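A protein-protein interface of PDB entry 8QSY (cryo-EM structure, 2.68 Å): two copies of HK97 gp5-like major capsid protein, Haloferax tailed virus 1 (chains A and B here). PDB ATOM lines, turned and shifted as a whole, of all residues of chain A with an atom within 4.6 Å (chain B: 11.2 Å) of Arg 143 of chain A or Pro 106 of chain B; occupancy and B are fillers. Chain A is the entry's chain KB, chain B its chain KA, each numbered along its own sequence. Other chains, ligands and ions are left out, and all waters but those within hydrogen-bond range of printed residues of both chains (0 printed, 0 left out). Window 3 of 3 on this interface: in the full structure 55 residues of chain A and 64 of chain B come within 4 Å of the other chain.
Thr 142 of chain A touches four residues of chain B.
Arg 143 of chain A touches just these residues of chain B: Asp 105 and Pro 106.
Gly 145 of chain A touches just one residue of chain B: Gln 116 (3.1 Å).
Printed residues of chain B within 4 Å of Trp 177 of chain A: Gln 116.
Tyr 353 of chain A touches none of the printed residues of chain B.
No residue of chain B comes within 4 Å of His 380 of chain A.
Phe 101 of chain B touches none of the printed residues of chain A.
Of the printed residues of chain A, Asp 105 of chain B touches Arg 143 (2.7 Å).
Of the printed residues of chain A, Pro 106 of chain B touches Arg 143.
Thr 111 of chain B touches none of the printed residues of chain A.
Printed residues of chain A within 4 Å of Arg 114 of chain B: Thr 142.
The nearest residue of chain B that does not touch Arg 143 of chain A is Phe 113 of chain B (5.9 Å).
The side-chain carboxylate of Asp 105 of chain B is in salt-bridge range of the guanidinium group of Arg 143 of chain A.
The backbone NH (N) of Gln 116 of chain B is in hydrogen-bond range of the side-chain hydroxyl (OG1) of Thr 142 of chain A (2.9 Å).
Hydrophobic or aromatic side chains of chain A within 4 Å of the printed part of chain B: Val 144 and Trp 177.
Printed residues of chain B that touch a printed residue of chain A: Asp 105, Pro 106, Phe 113, Arg 114, Glu 115 and Gln 116.
Among the printed residues, Asp or Glu carboxylates within 4 Å of a Lys or Arg side-chain nitrogen of the other chain: Arg 143 of chain A with Asp 105 of chain B (2.7 Å).
CG2 of Thr 142 of chain A touches CD2 of Phe 113 of chain B, at 3.9 Å.
CG2 of Thr 142 of chain A touches O of Arg 114 of chain B, 3.98 Å away.
C of Glu 115 of chain B touches OG1 of Thr 142 of chain A (3.8 Å).
CD of Pro 106 of chain B touches NH2 of Arg 143 of chain A, 3.9 Å away.
Glu 115 of chain B touches Val 144 of chain A.
Gln 116 of chain B touches Val 144 of chain A (N to O, 3.6 Å).
Gln 116 of chain B touches Gly 145 of chain A.
CZ2 of Trp 177 of chain A touches OE1 of Gln 116 of chain B, 3.3 Å away.
No position is printed for both chains.
Of the 10 pairs that touch across the chains among the printed residues, none has its exchanged pair printed and touching as well.
OD1 of Asp 110 of chain B is in salt-bridge range of NH2 of Arg 114 of chain B (3.3 Å).
The side-chain hydroxyl of Thr 142 of chain A sits at hydrogen-bond distance from the backbone carbonyl oxygen of Val 144 of chain A (2.6 Å).
O of Thr 142 of chain A sits at hydrogen-bond distance from NE1 of Trp 177 of chain A, at 3.1 Å.
The guanidinium group (NH1) of Arg 143 of chain A lies within hydrogen-bond range of the side-chain amide oxygen (OD1) of Asn 178 of chain A, at 2.9 Å.
The backbone carbonyl oxygen (O) of Arg 143 of chain A lies within hydrogen-bond range of the backbone NH (N) of Ala 179 of chain A, at 2.9 Å.
The backbone carbonyl oxygen (O) of Gly 145 of chain A lies within hydrogen-bond range of the backbone NH (N) of Trp 177 of chain A.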
ATOM      1  N   THR A 142     -22.037   4.587  26.970  1.00  0.00           N
ATOM      2  CA  THR A 142     -22.382   3.217  27.335  1.00  0.00           C
ATOM      3  C   THR A 142     -21.259   2.560  28.138  1.00  0.00           C
ATOM      4  O   THR A 142     -20.081   2.842  27.943  1.00  0.00           O
ATOM      5  CB  THR A 142     -22.733   2.369  26.102  1.00  0.00           C
ATOM      6  OG1 THR A 142     -21.640   2.364  25.185  1.00  0.00           O
ATOM      7  CG2 THR A 142     -23.987   2.809  25.378  1.00  0.00           C
ATOM      8  N   ARG A 143     -21.640   1.627  29.018  1.00  0.00           N
ATOM      9  CA  ARG A 143     -20.752   0.935  29.941  1.00  0.00           C
ATOM     10  C   ARG A 143     -19.682   0.122  29.205  1.00  0.00           C
ATOM     11  O   ARG A 143     -18.554  -0.019  29.685  1.00  0.00           O
ATOM     12  CB  ARG A 143     -21.604   0.020  30.819  1.00  0.00           C
ATOM     13  CG  ARG A 143     -21.026  -0.234  32.200  1.00  0.00           C
ATOM     14  CD  ARG A 143     -21.592  -1.512  32.799  1.00  0.00           C
ATOM     15  NE  ARG A 143     -20.782  -2.632  32.350  1.00  0.00           N
ATOM     16  CZ  ARG A 143     -21.202  -3.736  31.739  1.00  0.00           C
ATOM     17  NH1 ARG A 143     -20.306  -4.642  31.385  1.00  0.00           N
ATOM     18  NH2 ARG A 143     -22.481  -3.951  31.480  1.00  0.00           N
ATOM     19  N   VAL A 144     -20.050  -0.408  28.030  1.00  0.00           N
ATOM     20  CA  VAL A 144     -19.158  -1.133  27.133  1.00  0.00           C
ATOM     21  C   VAL A 144     -19.053  -0.336  25.834  1.00  0.00           C
ATOM     22  O   VAL A 144     -20.005   0.337  25.442  1.00  0.00           O
ATOM     23  CB  VAL A 144     -19.679  -2.564  26.881  1.00  0.00           C
ATOM     24  CG1 VAL A 144     -18.816  -3.341  25.896  1.00  0.00           C
ATOM     25  CG2 VAL A 144     -19.797  -3.332  28.181  1.00  0.00           C
ATOM     26  N   GLY A 145     -17.894  -0.402  25.177  1.00  0.00           N
ATOM     27  CA  GLY A 145     -17.694   0.258  23.904  1.00  0.00           C
ATOM     28  C   GLY A 145     -16.351  -0.080  23.269  1.00  0.00           C
ATOM     29  O   GLY A 145     -15.617  -0.930  23.753  1.00  0.00           O
ATOM     30  N   TRP A 177     -13.414  -1.006  25.626  1.00  0.00           N
ATOM     31  CA  TRP A 177     -13.605  -0.700  27.035  1.00  0.00           C
ATOM     32  C   TRP A 177     -14.779  -1.484  27.601  1.00  0.00           C
ATOM     33  O   TRP A 177     -15.785  -1.676  26.937  1.00  0.00           O
ATOM     34  CB  TRP A 177     -13.756   0.799  27.276  1.00  0.00           C
ATOM     35  CG  TRP A 177     -15.060   1.462  26.953  1.00  0.00           C
ATOM     36  CD1 TRP A 177     -16.200   1.463  27.701  1.00  0.00           C
ATOM     37  CD2 TRP A 177     -15.321   2.333  25.829  1.00  0.00           C
ATOM     38  NE1 TRP A 177     -17.142   2.274  27.119  1.00  0.00           N
ATOM     39  CE2 TRP A 177     -16.627   2.858  25.987  1.00  0.00           C
ATOM     40  CE3 TRP A 177     -14.569   2.763  24.726  1.00  0.00           C
ATOM     41  CZ2 TRP A 177     -17.185   3.773  25.074  1.00  0.00           C
ATOM     42  CZ3 TRP A 177     -15.104   3.680  23.833  1.00  0.00           C
ATOM     43  CH2 TRP A 177     -16.398   4.190  24.016  1.00  0.00           C
ATOM     44  N   ASN A 178     -14.656  -1.876  28.863  1.00  0.00           N
ATOM     45  CA  ASN A 178     -15.726  -2.519  29.597  1.00  0.00           C
ATOM     46  C   ASN A 178     -15.652  -2.004  31.031  1.00  0.00           C
ATOM     47  O   ASN A 178     -14.933  -2.561  31.858  1.00  0.00           O
ATOM     48  CB  ASN A 178     -15.597  -4.036  29.460  1.00  0.00           C
ATOM     49  CG  ASN A 178     -16.767  -4.794  30.046  1.00  0.00           C
ATOM     50  OD1 ASN A 178     -17.477  -4.309  30.925  1.00  0.00           O
ATOM     51  ND2 ASN A 178     -16.999  -5.995  29.544  1.00  0.00           N
ATOM     52  N   ALA A 179     -16.337  -0.888  31.288  1.00  0.00           N
ATOM     53  CA  ALA A 179     -16.229  -0.171  32.549  1.00  0.00           C
ATOM     54  C   ALA A 179     -16.784  -1.017  33.699  1.00  0.00           C
ATOM     55  O   ALA A 179     -17.957  -1.375  33.710  1.00  0.00           O
ATOM     56  CB  ALA A 179     -16.909   1.170  32.392  1.00  0.00           C
ATOM     57  N   TYR A 353     -18.099   5.975  33.076  1.00  0.00           N
ATOM     58  CA  TYR A 353     -19.510   5.843  32.743  1.00  0.00           C
ATOM     59  C   TYR A 353     -20.355   5.957  34.017  1.00  0.00           C
ATOM     60  O   TYR A 353     -20.055   5.328  35.026  1.00  0.00           O
ATOM     61  CB  TYR A 353     -19.763   4.571  31.918  1.00  0.00           C
ATOM     62  CG  TYR A 353     -21.234   4.254  31.811  1.00  0.00           C
ATOM     63  CD1 TYR A 353     -22.055   4.914  30.897  1.00  0.00           C
ATOM     64  CD2 TYR A 353     -21.815   3.341  32.679  1.00  0.00           C
ATOM     65  CE1 TYR A 353     -23.425   4.693  30.871  1.00  0.00           C
ATOM     66  CE2 TYR A 353     -23.181   3.097  32.645  1.00  0.00           C
ATOM     67  CZ  TYR A 353     -23.990   3.784  31.756  1.00  0.00           C
ATOM     68  OH  TYR A 353     -25.337   3.552  31.796  1.00  0.00           O
ATOM     69  N   HIS A 380     -18.594   3.703  37.095  1.00  0.00           N
ATOM     70  CA  HIS A 380     -18.017   2.644  36.282  1.00  0.00           C
ATOM     71  C   HIS A 380     -16.752   3.186  35.628  1.00  0.00           C
ATOM     72  O   HIS A 380     -16.788   4.267  35.048  1.00  0.00           O
ATOM     73  CB  HIS A 380     -19.017   2.160  35.231  1.00  0.00           C
ATOM     74  CG  HIS A 380     -20.326   1.687  35.756  1.00  0.00           C
ATOM     75  ND1 HIS A 380     -20.732   0.357  35.737  1.00  0.00           N
ATOM     76  CD2 HIS A 380     -21.362   2.406  36.231  1.00  0.00           C
ATOM     77  CE1 HIS A 380     -21.969   0.288  36.191  1.00  0.00           C
ATOM     78  NE2 HIS A 380     -22.371   1.529  36.504  1.00  0.00           N
ATOM     79  N   PHE B 101     -33.459 -12.548  35.364  1.00  0.00           N
ATOM     80  CA  PHE B 101     -33.117 -11.426  36.290  1.00  0.00           C
ATOM     81  C   PHE B 101     -33.469 -10.084  35.656  1.00  0.00           C
ATOM     82  O   PHE B 101     -32.806  -9.656  34.715  1.00  0.00           O
ATOM     83  CB  PHE B 101     -31.621 -11.419  36.629  1.00  0.00           C
ATOM     84  CG  PHE B 101     -31.104 -10.113  37.198  1.00  0.00           C
ATOM     85  CD1 PHE B 101     -31.550  -9.644  38.430  1.00  0.00           C
ATOM     86  CD2 PHE B 101     -30.173  -9.340  36.506  1.00  0.00           C
ATOM     87  CE1 PHE B 101     -31.081  -8.448  38.960  1.00  0.00           C
ATOM     88  CE2 PHE B 101     -29.698  -8.146  37.042  1.00  0.00           C
ATOM     89  CZ  PHE B 101     -30.154  -7.703  38.264  1.00  0.00           C
ATOM     90  N   ALA B 102     -34.467  -9.398  36.229  1.00  0.00           N
ATOM     91  CA  ALA B 102     -34.689  -7.971  36.017  1.00  0.00           C
ATOM     92  C   ALA B 102     -34.561  -7.576  34.534  1.00  0.00           C
ATOM     93  O   ALA B 102     -35.203  -8.183  33.663  1.00  0.00           O
ATOM     94  CB  ALA B 102     -33.781  -7.188  36.959  1.00  0.00           C
ATOM     95  N   ALA B 103     -33.802  -6.503  34.263  1.00  0.00           N
ATOM     96  CA  ALA B 103     -33.345  -6.117  32.938  1.00  0.00           C
ATOM     97  C   ALA B 103     -32.042  -5.350  33.142  1.00  0.00           C
ATOM     98  O   ALA B 103     -32.041  -4.282  33.753  1.00  0.00           O
ATOM     99  CB  ALA B 103     -34.380  -5.271  32.231  1.00  0.00           C
ATOM    100  N   SER B 104     -30.935  -5.930  32.666  1.00  0.00           N
ATOM    101  CA  SER B 104     -29.604  -5.388  32.875  1.00  0.00           C
ATOM    102  C   SER B 104     -28.886  -5.279  31.531  1.00  0.00           C
ATOM    103  O   SER B 104     -29.100  -6.094  30.639  1.00  0.00           O
ATOM    104  CB  SER B 104     -28.856  -6.244  33.871  1.00  0.00           C
ATOM    105  OG  SER B 104     -28.611  -7.546  33.360  1.00  0.00           O
ATOM    106  N   ASP B 105     -27.986  -4.303  31.396  1.00  0.00           N
ATOM    107  CA  ASP B 105     -27.439  -4.002  30.082  1.00  0.00           C
ATOM    108  C   ASP B 105     -26.615  -5.131  29.446  1.00  0.00           C
ATOM    109  O   ASP B 105     -26.630  -5.216  28.220  1.00  0.00           O
ATOM    110  CB  ASP B 105     -26.788  -2.619  30.005  1.00  0.00           C
ATOM    111  CG  ASP B 105     -25.358  -2.582  30.512  1.00  0.00           C
ATOM    112  OD1 ASP B 105     -25.094  -3.170  31.572  1.00  0.00           O
ATOM    113  OD2 ASP B 105     -24.514  -1.936  29.855  1.00  0.00           O
ATOM    114  N   PRO B 106     -25.918  -6.071  30.148  1.00  0.00           N
ATOM    115  CA  PRO B 106     -25.269  -7.184  29.448  1.00  0.00           C
ATOM    116  C   PRO B 106     -26.229  -8.201  28.824  1.00  0.00           C
ATOM    117  O   PRO B 106     -25.789  -9.050  28.065  1.00  0.00           O
ATOM    118  CB  PRO B 106     -24.388  -7.843  30.520  1.00  0.00           C
ATOM    119  CG  PRO B 106     -25.150  -7.581  31.786  1.00  0.00           C
ATOM    120  CD  PRO B 106     -25.682  -6.174  31.600  1.00  0.00           C
ATOM    121  N   GLU B 107     -27.537  -8.101  29.098  1.00  0.00           N
ATOM    122  CA  GLU B 107     -28.529  -8.970  28.469  1.00  0.00           C
ATOM    123  C   GLU B 107     -29.030  -8.406  27.139  1.00  0.00           C
ATOM    124  O   GLU B 107     -29.401  -9.168  26.249  1.00  0.00           O
ATOM    125  CB  GLU B 107     -29.745  -9.135  29.370  1.00  0.00           C
ATOM    126  CG  GLU B 107     -29.412  -9.781  30.691  1.00  0.00           C
ATOM    127  CD  GLU B 107     -30.601  -9.706  31.619  1.00  0.00           C
ATOM    128  OE1 GLU B 107     -30.734  -8.676  32.321  1.00  0.00           O
ATOM    129  OE2 GLU B 107     -31.408 -10.659  31.613  1.00  0.00           O
ATOM    130  N   TYR B 108     -29.061  -7.071  27.019  1.00  0.00           N
ATOM    131  CA  TYR B 108     -29.757  -6.370  25.945  1.00  0.00           C
ATOM    132  C   TYR B 108     -28.839  -5.457  25.124  1.00  0.00           C
ATOM    133  O   TYR B 108     -29.323  -4.630  24.353  1.00  0.00           O
ATOM    134  CB  TYR B 108     -30.979  -5.649  26.525  1.00  0.00           C
ATOM    135  CG  TYR B 108     -32.004  -6.566  27.156  1.00  0.00           C
ATOM    136  CD1 TYR B 108     -32.443  -7.709  26.498  1.00  0.00           C
ATOM    137  CD2 TYR B 108     -32.570  -6.282  28.394  1.00  0.00           C
ATOM    138  CE1 TYR B 108     -33.399  -8.550  27.052  1.00  0.00           C
ATOM    139  CE2 TYR B 108     -33.520  -7.119  28.970  1.00  0.00           C
ATOM    140  CZ  TYR B 108     -33.940  -8.255  28.292  1.00  0.00           C
ATOM    141  OH  TYR B 108     -34.875  -9.090  28.840  1.00  0.00           O
ATOM    142  N   VAL B 109     -27.525  -5.674  25.236  1.00  0.00           N
ATOM    143  CA  VAL B 109     -26.450  -4.907  24.613  1.00  0.00           C
ATOM    144  C   VAL B 109     -26.484  -4.897  23.077  1.00  0.00           C
ATOM    145  O   VAL B 109     -25.798  -4.073  22.469  1.00  0.00           O
ATOM    146  CB  VAL B 109     -25.098  -5.397  25.163  1.00  0.00           C
ATOM    147  CG1 VAL B 109     -24.827  -6.847  24.796  1.00  0.00           C
ATOM    148  CG2 VAL B 109     -23.933  -4.510  24.759  1.00  0.00           C
ATOM    149  N   ASP B 110     -27.279  -5.780  22.451  1.00  0.00           N
ATOM    150  CA  ASP B 110     -27.517  -5.748  21.009  1.00  0.00           C
ATOM    151  C   ASP B 110     -29.012  -5.801  20.663  1.00  0.00           C
ATOM    152  O   ASP B 110     -29.370  -6.121  19.528  1.00  0.00           O
ATOM    153  CB  ASP B 110     -26.746  -6.869  20.306  1.00  0.00           C
ATOM    154  CG  ASP B 110     -25.238  -6.686  20.296  1.00  0.00           C
ATOM    155  OD1 ASP B 110     -24.778  -5.688  19.705  1.00  0.00           O
ATOM    156  OD2 ASP B 110     -24.530  -7.577  20.833  1.00  0.00           O
ATOM    157  N   THR B 111     -29.903  -5.485  21.624  1.00  0.00           N
ATOM    158  CA  THR B 111     -31.343  -5.600  21.413  1.00  0.00           C
ATOM    159  C   THR B 111     -32.130  -4.378  21.891  1.00  0.00           C
ATOM    160  O   THR B 111     -33.291  -4.245  21.519  1.00  0.00           O
ATOM    161  CB  THR B 111     -31.952  -6.852  22.057  1.00  0.00           C
ATOM    162  OG1 THR B 111     -32.110  -6.621  23.454  1.00  0.00           O
ATOM    163  CG2 THR B 111     -31.158  -8.123  21.856  1.00  0.00           C
ATOM    164  N   LEU B 112     -31.545  -3.512  22.732  1.00  0.00           N
ATOM    165  CA  LEU B 112     -32.215  -2.288  23.170  1.00  0.00           C
ATOM    166  C   LEU B 112     -31.338  -1.043  23.000  1.00  0.00           C
ATOM    167  O   LEU B 112     -31.837   0.076  23.120  1.00  0.00           O
ATOM    168  CB  LEU B 112     -32.666  -2.427  24.624  1.00  0.00           C
ATOM    169  CG  LEU B 112     -33.806  -3.405  24.896  1.00  0.00           C
ATOM    170  CD1 LEU B 112     -34.063  -3.476  26.386  1.00  0.00           C
ATOM    171  CD2 LEU B 112     -35.086  -2.966  24.193  1.00  0.00           C
ATOM    172  N   PHE B 113     -30.048  -1.249  22.703  1.00  0.00           N
ATOM    173  CA  PHE B 113     -29.083  -0.207  22.382  1.00  0.00           C
ATOM    174  C   PHE B 113     -27.896  -0.864  21.678  1.00  0.00           C
ATOM    175  O   PHE B 113     -27.785  -2.085  21.687  1.00  0.00           O
ATOM    176  CB  PHE B 113     -28.654   0.535  23.651  1.00  0.00           C
ATOM    177  CG  PHE B 113     -27.818  -0.275  24.614  1.00  0.00           C
ATOM    178  CD1 PHE B 113     -28.403  -1.192  25.484  1.00  0.00           C
ATOM    179  CD2 PHE B 113     -26.438  -0.114  24.655  1.00  0.00           C
ATOM    180  CE1 PHE B 113     -27.625  -1.943  26.361  1.00  0.00           C
ATOM    181  CE2 PHE B 113     -25.664  -0.856  25.537  1.00  0.00           C
ATOM    182  CZ  PHE B 113     -26.257  -1.773  26.380  1.00  0.00           C
ATOM    183  N   ARG B 114     -27.020  -0.054  21.058  1.00  0.00           N
ATOM    184  CA  ARG B 114     -25.734  -0.505  20.536  1.00  0.00           C
ATOM    185  C   ARG B 114     -24.627   0.064  21.419  1.00  0.00           C
ATOM    186  O   ARG B 114     -24.668   1.235  21.791  1.00  0.00           O
ATOM    187  CB  ARG B 114     -25.543  -0.015  19.092  1.00  0.00           C
ATOM    188  CG  ARG B 114     -25.658  -1.091  18.020  1.00  0.00           C
ATOM    189  CD  ARG B 114     -27.031  -1.721  17.992  1.00  0.00           C
ATOM    190  NE  ARG B 114     -27.385  -2.466  16.798  1.00  0.00           N
ATOM    191  CZ  ARG B 114     -27.440  -3.790  16.709  1.00  0.00           C
ATOM    192  NH1 ARG B 114     -27.813  -4.344  15.570  1.00  0.00           N
ATOM    193  NH2 ARG B 114     -27.142  -4.561  17.747  1.00  0.00           N
ATOM    194  N   GLU B 115     -23.625  -0.762  21.748  1.00  0.00           N
ATOM    195  CA  GLU B 115     -22.479  -0.278  22.512  1.00  0.00           C
ATOM    196  C   GLU B 115     -21.747   0.813  21.718  1.00  0.00           C
ATOM    197  O   GLU B 115     -21.658   0.734  20.499  1.00  0.00           O
ATOM    198  CB  GLU B 115     -21.618  -1.453  22.994  1.00  0.00           C
ATOM    199  CG  GLU B 115     -20.731  -2.076  21.931  1.00  0.00           C
ATOM    200  CD  GLU B 115     -20.050  -3.382  22.322  1.00  0.00           C
ATOM    201  OE1 GLU B 115     -20.710  -4.240  22.941  1.00  0.00           O
ATOM    202  OE2 GLU B 115     -18.855  -3.544  22.001  1.00  0.00           O
ATOM    203  N   GLN B 116     -21.222   1.839  22.405  1.00  0.00           N
ATOM    204  CA  GLN B 116     -20.654   3.008  21.744  1.00  0.00           C
ATOM    205  C   GLN B 116     -19.412   2.645  20.921  1.00  0.00           C
ATOM    206  O   GLN B 116     -18.586   1.836  21.337  1.00  0.00           O
ATOM    207  CB  GLN B 116     -20.318   4.069  22.791  1.00  0.00           C
ATOM    208  CG  GLN B 116     -19.692   5.341  22.223  1.00  0.00           C
ATOM    209  CD  GLN B 116     -19.415   6.393  23.274  1.00  0.00           C
ATOM    210  OE1 GLN B 116     -19.422   6.125  24.474  1.00  0.00           O
ATOM    211  NE2 GLN B 116     -19.159   7.615  22.832  1.00  0.00           N
ATOM    212  N   LEU B 117     -19.299   3.238  19.725  1.00  0.00           N
ATOM    213  CA  LEU B 117     -18.051   3.232  18.980  1.00  0.00           C
ATOM    214  C   LEU B 117     -17.529   4.666  18.928  1.00  0.00           C
ATOM    215  O   LEU B 117     -18.226   5.557  18.449  1.00  0.00           O
ATOM    216  CB  LEU B 117     -18.302   2.656  17.583  1.00  0.00           C
ATOM    217  CG  LEU B 117     -17.062   2.526  16.704  1.00  0.00           C
ATOM    218  CD1 LEU B 117     -16.102   1.479  17.248  1.00  0.00           C
ATOM    219  CD2 LEU B 117     -17.462   2.184  15.286  1.00  0.00           C
